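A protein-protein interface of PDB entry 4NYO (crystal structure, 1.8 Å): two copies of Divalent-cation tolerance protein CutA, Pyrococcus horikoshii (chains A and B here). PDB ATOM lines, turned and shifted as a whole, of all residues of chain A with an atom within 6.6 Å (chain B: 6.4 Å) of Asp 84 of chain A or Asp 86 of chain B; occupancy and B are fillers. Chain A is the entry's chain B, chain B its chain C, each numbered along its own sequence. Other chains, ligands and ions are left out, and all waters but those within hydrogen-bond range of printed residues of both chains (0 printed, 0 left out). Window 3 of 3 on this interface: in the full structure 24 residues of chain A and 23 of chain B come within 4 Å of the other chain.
CG1 of Val 85 of chain B touches CG2 of Ile 81 of chain A, 3.6 Å away. Ile 81 of chain A touches Asp 87 of chain B. Arg 82 of chain A touches Val 85 of chain B (O to CG1, 3.7 Å). Ile 83 of chain A touches Asp 86 of chain B.
Asp 84 of chain A touches just one residue of chain B: Asp 86. Asp 86 of chain B touches three residues of chain A. Printed residues of chain A within 4 Å of Val 85 of chain B: Ile 81 and Arg 82. Of the printed residues of chain A, Asp 87 of chain B touches Ile 81 and Arg 82. The nearest residue of chain A that does not touch Asp 86 of chain B is Val 85 of chain A (5.6 Å). The nearest printed residue of chain A that does not touch Asp 87 of chain B is Ile 83 of chain A (5.3 Å).
Of the 11 printed residues of chain A, 4 touch a printed residue of chain B. Hydrophobic or aromatic side chains of chain A within 4 Å of the printed part of chain B: Ile 81. Printed residues of chain B that touch a printed residue of chain A: Val 85, Asp 86 and Asp 87. Hydrophobic or aromatic side chains of chain B within 4 Å of the printed part of chain A: Val 85.
Asp 84 of chain A touches Asp 86 of chain B, but with the chains exchanged Asp 86 of chain A does not touch Asp 84 of chain B (8.0 Å). Positions printed for both chains: 1, 84, 85, 86 and 87. Of the 7 pairs that touch across the chains among the printed residues, none has its exchanged pair printed and touching as well.
The side-chain carboxylate (OD2) of Asp 86 of chain B sits at hydrogen-bond distance from the backbone NH (N) of Asp 84 of chain A (2.5 Å). O of Arg 82 of chain A lies within hydrogen-bond range of N of Asp 86 of chain B (3.0 Å). The backbone NH (N) of Arg 82 of chain A is in hydrogen-bond range of the backbone carbonyl oxygen (O) of Asp 87 of chain B, 2.8 Å away.
N of Val 85 of chain B sits at hydrogen-bond distance from O of Met 1 of chain B (3.0 Å). The backbone carbonyl oxygen (O) of Ile 3 of chain A is in hydrogen-bond range of the backbone NH (N) of Ile 83 of chain A, at 2.8 Å. The guanidinium group of Arg 82 of chain A is in salt-bridge range of the side-chain carboxylate of Asp 84 of chain A, at 2.7 Å. The side-chain carboxylate of Glu 59 of chain A lies within salt-bridge range of the guanidinium group of Arg 82 of chain A, at 2.8 Å.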
ATOM      1  N   MET A   1      -1.262 -30.626  -7.073  1.00  0.00           N
ATOM      2  CA  MET A   1      -0.648 -30.760  -8.429  1.00  0.00           C
ATOM      3  C   MET A   1      -1.350 -29.855  -9.435  1.00  0.00           C
ATOM      4  O   MET A   1      -2.341 -29.196  -9.115  1.00  0.00           O
ATOM      5  CB  MET A   1      -0.736 -32.208  -8.921  1.00  0.00           C
ATOM      6  CG  MET A   1      -2.157 -32.706  -9.130  1.00  0.00           C
ATOM      7  SD  MET A   1      -2.205 -34.291  -9.983  1.00  0.00           S
ATOM      8  CE  MET A   1      -1.913 -33.766 -11.660  1.00  0.00           C
ATOM      9  N   ILE A   2      -0.834 -29.826 -10.655  1.00  0.00           N
ATOM     10  CA  ILE A   2      -1.434 -29.002 -11.690  1.00  0.00           C
ATOM     11  C   ILE A   2      -1.470 -29.727 -13.024  1.00  0.00           C
ATOM     12  O   ILE A   2      -0.746 -30.692 -13.245  1.00  0.00           O
ATOM     13  CB  ILE A   2      -0.656 -27.663 -11.885  1.00  0.00           C
ATOM     14  CG1 ILE A   2       0.771 -27.947 -12.364  1.00  0.00           C
ATOM     15  CG2 ILE A   2      -0.638 -26.874 -10.577  1.00  0.00           C
ATOM     16  CD1 ILE A   2       1.572 -26.687 -12.712  1.00  0.00           C
ATOM     17  N   ILE A   3      -2.345 -29.257 -13.901  1.00  0.00           N
ATOM     18  CA  ILE A   3      -2.455 -29.790 -15.241  1.00  0.00           C
ATOM     19  C   ILE A   3      -2.051 -28.611 -16.117  1.00  0.00           C
ATOM     20  O   ILE A   3      -2.482 -27.486 -15.872  1.00  0.00           O
ATOM     21  CB  ILE A   3      -3.911 -30.173 -15.594  1.00  0.00           C
ATOM     22  CG1 ILE A   3      -4.353 -31.390 -14.778  1.00  0.00           C
ATOM     23  CG2 ILE A   3      -4.026 -30.440 -17.088  1.00  0.00           C
ATOM     24  CD1 ILE A   3      -3.573 -32.649 -15.073  1.00  0.00           C
ATOM     25  N   GLU A  59       2.855 -28.313  -8.553  1.00  0.00           N
ATOM     26  CA  GLU A  59       2.533 -26.897  -8.551  1.00  0.00           C
ATOM     27  C   GLU A  59       3.786 -26.022  -8.511  1.00  0.00           C
ATOM     28  O   GLU A  59       3.876 -25.022  -9.221  1.00  0.00           O
ATOM     29  CB  GLU A  59       1.636 -26.596  -7.350  1.00  0.00           C
ATOM     30  CG  GLU A  59       1.114 -25.180  -7.268  1.00  0.00           C
ATOM     31  CD  GLU A  59      -0.084 -25.076  -6.343  1.00  0.00           C
ATOM     32  OE1 GLU A  59       0.002 -25.568  -5.197  1.00  0.00           O
ATOM     33  OE2 GLU A  59      -1.113 -24.507  -6.761  1.00  0.00           O
ATOM     34  N   ILE A  81      -1.330 -23.093 -20.673  1.00  0.00           N
ATOM     35  CA  ILE A  81      -2.404 -22.916 -19.709  1.00  0.00           C
ATOM     36  C   ILE A  81      -2.331 -23.820 -18.484  1.00  0.00           C
ATOM     37  O   ILE A  81      -2.319 -25.043 -18.601  1.00  0.00           O
ATOM     38  CB  ILE A  81      -3.742 -23.133 -20.437  1.00  0.00           C
ATOM     39  CG1 ILE A  81      -3.865 -22.102 -21.566  1.00  0.00           C
ATOM     40  CG2 ILE A  81      -4.897 -23.048 -19.468  1.00  0.00           C
ATOM     41  CD1 ILE A  81      -4.995 -22.377 -22.550  1.00  0.00           C
ATOM     42  N   ARG A  82      -2.305 -23.197 -17.308  1.00  0.00           N
ATOM     43  CA  ARG A  82      -2.227 -23.933 -16.052  1.00  0.00           C
ATOM     44  C   ARG A  82      -3.566 -24.011 -15.330  1.00  0.00           C
ATOM     45  O   ARG A  82      -4.223 -22.996 -15.094  1.00  0.00           O
ATOM     46  CB  ARG A  82      -1.204 -23.284 -15.117  1.00  0.00           C
ATOM     47  CG  ARG A  82      -1.290 -23.792 -13.684  1.00  0.00           C
ATOM     48  CD  ARG A  82      -0.382 -23.003 -12.756  1.00  0.00           C
ATOM     49  NE  ARG A  82      -0.627 -23.360 -11.363  1.00  0.00           N
ATOM     50  CZ  ARG A  82       0.043 -22.866 -10.327  1.00  0.00           C
ATOM     51  NH1 ARG A  82       1.012 -21.983 -10.521  1.00  0.00           N
ATOM     52  NH2 ARG A  82      -0.258 -23.258  -9.095  1.00  0.00           N
ATOM     53  N   ILE A  83      -3.960 -25.228 -14.978  1.00  0.00           N
ATOM     54  CA  ILE A  83      -5.197 -25.450 -14.251  1.00  0.00           C
ATOM     55  C   ILE A  83      -4.840 -26.209 -12.977  1.00  0.00           C
ATOM     56  O   ILE A  83      -4.314 -27.317 -13.034  1.00  0.00           O
ATOM     57  CB  ILE A  83      -6.194 -26.287 -15.072  1.00  0.00           C
ATOM     58  CG1 ILE A  83      -6.523 -25.570 -16.385  1.00  0.00           C
ATOM     59  CG2 ILE A  83      -7.459 -26.517 -14.262  1.00  0.00           C
ATOM     60  CD1 ILE A  83      -7.434 -26.361 -17.305  1.00  0.00           C
ATOM     61  N   ASP A  84      -5.107 -25.600 -11.828  1.00  0.00           N
ATOM     62  CA  ASP A  84      -4.809 -26.239 -10.552  1.00  0.00           C
ATOM     63  C   ASP A  84      -5.781 -27.380 -10.293  1.00  0.00           C
ATOM     64  O   ASP A  84      -6.980 -27.260 -10.557  1.00  0.00           O
ATOM     65  CB  ASP A  84      -4.914 -25.224  -9.416  1.00  0.00           C
ATOM     66  CG  ASP A  84      -3.765 -24.244  -9.402  1.00  0.00           C
ATOM     67  OD1 ASP A  84      -3.110 -24.064 -10.449  1.00  0.00           O
ATOM     68  OD2 ASP A  84      -3.524 -23.640  -8.341  1.00  0.00           O
ATOM     69  N   VAL A  85      -5.259 -28.488  -9.777  1.00  0.00           N
ATOM     70  CA  VAL A  85      -6.083 -29.643  -9.462  1.00  0.00           C
ATOM     71  C   VAL A  85      -6.562 -29.465  -8.027  1.00  0.00           C
ATOM     72  O   VAL A  85      -5.758 -29.330  -7.104  1.00  0.00           O
ATOM     73  CB  VAL A  85      -5.280 -30.950  -9.598  1.00  0.00           C
ATOM     74  CG1 VAL A  85      -6.094 -32.129  -9.094  1.00  0.00           C
ATOM     75  CG2 VAL A  85      -4.893 -31.159 -11.050  1.00  0.00           C
ATOM     76  N   ASP A  86      -7.875 -29.447  -7.850  1.00  0.00           N
ATOM     77  CA  ASP A  86      -8.467 -29.254  -6.533  1.00  0.00           C
ATOM     78  C   ASP A  86      -8.270 -30.431  -5.591  1.00  0.00           C
ATOM     79  O   ASP A  86      -8.251 -30.257  -4.374  1.00  0.00           O
ATOM     80  CB  ASP A  86      -9.943 -28.920  -6.693  1.00  0.00           C
ATOM     81  CG  ASP A  86     -10.145 -27.624  -7.446  1.00  0.00           C
ATOM     82  OD1 ASP A  86      -9.882 -26.556  -6.853  1.00  0.00           O
ATOM     83  OD2 ASP A  86     -10.542 -27.675  -8.630  1.00  0.00           O
ATOM     84  N   ASP A  87      -8.126 -31.625  -6.157  1.00  0.00           N
ATOM     85  CA  ASP A  87      -7.889 -32.827  -5.361  1.00  0.00           C
ATOM     86  C   ASP A  87      -7.560 -33.970  -6.307  1.00  0.00           C
ATOM     87  O   ASP A  87      -7.981 -33.976  -7.466  1.00  0.00           O
ATOM     88  CB  ASP A  87      -9.118 -33.199  -4.521  1.00  0.00           C
ATOM     89  CG  ASP A  87      -8.777 -34.148  -3.370  1.00  0.00           C
ATOM     90  OD1 ASP A  87      -9.702 -34.769  -2.809  1.00  0.00           O
ATOM     91  OD2 ASP A  87      -7.585 -34.265  -3.012  1.00  0.00           O
ATOM     92  N   MET B   1      -8.025 -15.403 -17.500  1.00  0.00           N
ATOM     93  CA  MET B   1      -8.778 -15.991 -18.642  1.00  0.00           C
ATOM     94  C   MET B   1      -9.509 -17.246 -18.189  1.00  0.00           C
ATOM     95  O   MET B   1      -9.310 -17.731 -17.069  1.00  0.00           O
ATOM     96  CB  MET B   1      -7.831 -16.340 -19.803  1.00  0.00           C
ATOM     97  CG  MET B   1      -6.887 -17.510 -19.538  1.00  0.00           C
ATOM     98  SD  MET B   1      -5.985 -18.046 -21.026  1.00  0.00           S
ATOM     99  CE  MET B   1      -7.244 -19.012 -21.859  1.00  0.00           C
ATOM    100  N   ASP B  84     -11.939 -21.701 -14.690  1.00  0.00           N
ATOM    101  CA  ASP B  84     -10.978 -20.605 -14.610  1.00  0.00           C
ATOM    102  C   ASP B  84      -9.546 -21.081 -14.784  1.00  0.00           C
ATOM    103  O   ASP B  84      -9.156 -22.130 -14.266  1.00  0.00           O
ATOM    104  CB  ASP B  84     -11.112 -19.888 -13.261  1.00  0.00           C
ATOM    105  CG  ASP B  84     -12.314 -18.956 -13.206  1.00  0.00           C
ATOM    106  OD1 ASP B  84     -13.315 -19.226 -13.894  1.00  0.00           O
ATOM    107  OD2 ASP B  84     -12.259 -17.957 -12.462  1.00  0.00           O
ATOM    108  N   VAL B  85      -8.762 -20.296 -15.515  1.00  0.00           N
ATOM    109  CA  VAL B  85      -7.358 -20.616 -15.737  1.00  0.00           C
ATOM    110  C   VAL B  85      -6.570 -19.961 -14.609  1.00  0.00           C
ATOM    111  O   VAL B  85      -6.645 -18.745 -14.405  1.00  0.00           O
ATOM    112  CB  VAL B  85      -6.889 -20.085 -17.113  1.00  0.00           C
ATOM    113  CG1 VAL B  85      -5.371 -20.223 -17.254  1.00  0.00           C
ATOM    114  CG2 VAL B  85      -7.592 -20.868 -18.217  1.00  0.00           C
ATOM    115  N   ASP B  86      -5.826 -20.776 -13.866  1.00  0.00           N
ATOM    116  CA  ASP B  86      -5.049 -20.286 -12.737  1.00  0.00           C
ATOM    117  C   ASP B  86      -3.858 -19.430 -13.151  1.00  0.00           C
ATOM    118  O   ASP B  86      -3.553 -18.425 -12.510  1.00  0.00           O
ATOM    119  CB  ASP B  86      -4.618 -21.477 -11.885  1.00  0.00           C
ATOM    120  CG  ASP B  86      -5.806 -22.202 -11.290  1.00  0.00           C
ATOM    121  OD1 ASP B  86      -6.398 -21.667 -10.333  1.00  0.00           O
ATOM    122  OD2 ASP B  86      -6.166 -23.290 -11.792  1.00  0.00           O
ATOM    123  N   ASP B  87      -3.190 -19.822 -14.227  1.00  0.00           N
ATOM    124  CA  ASP B  87      -2.065 -19.054 -14.733  1.00  0.00           C
ATOM    125  C   ASP B  87      -1.829 -19.441 -16.185  1.00  0.00           C
ATOM    126  O   ASP B  87      -2.250 -20.510 -16.635  1.00  0.00           O
ATOM    127  CB  ASP B  87      -0.807 -19.301 -13.893  1.00  0.00           C
ATOM    128  CG  ASP B  87       0.141 -18.108 -13.900  1.00  0.00           C
ATOM    129  OD1 ASP B  87       1.112 -18.112 -13.115  1.00  0.00           O
ATOM    130  OD2 ASP B  87      -0.086 -17.161 -14.688  1.00  0.00           O
ATOM    131  N   VAL B  88      -1.166 -18.562 -16.924  1.00  0.00           N
ATOM    132  CA  VAL B  88      -0.902 -18.808 -18.334  1.00  0.00           C
ATOM    133  C   VAL B  88       0.250 -17.901 -18.762  1.00  0.00           C
ATOM    134  O   VAL B  88       0.465 -16.847 -18.147  1.00  0.00           O
ATOM    135  CB  VAL B  88      -2.177 -18.495 -19.163  1.00  0.00           C
ATOM    136  CG1 VAL B  88      -2.687 -17.103 -18.818  1.00  0.00           C
ATOM    137  CG2 VAL B  88      -1.888 -18.611 -20.659  1.00  0.00           C
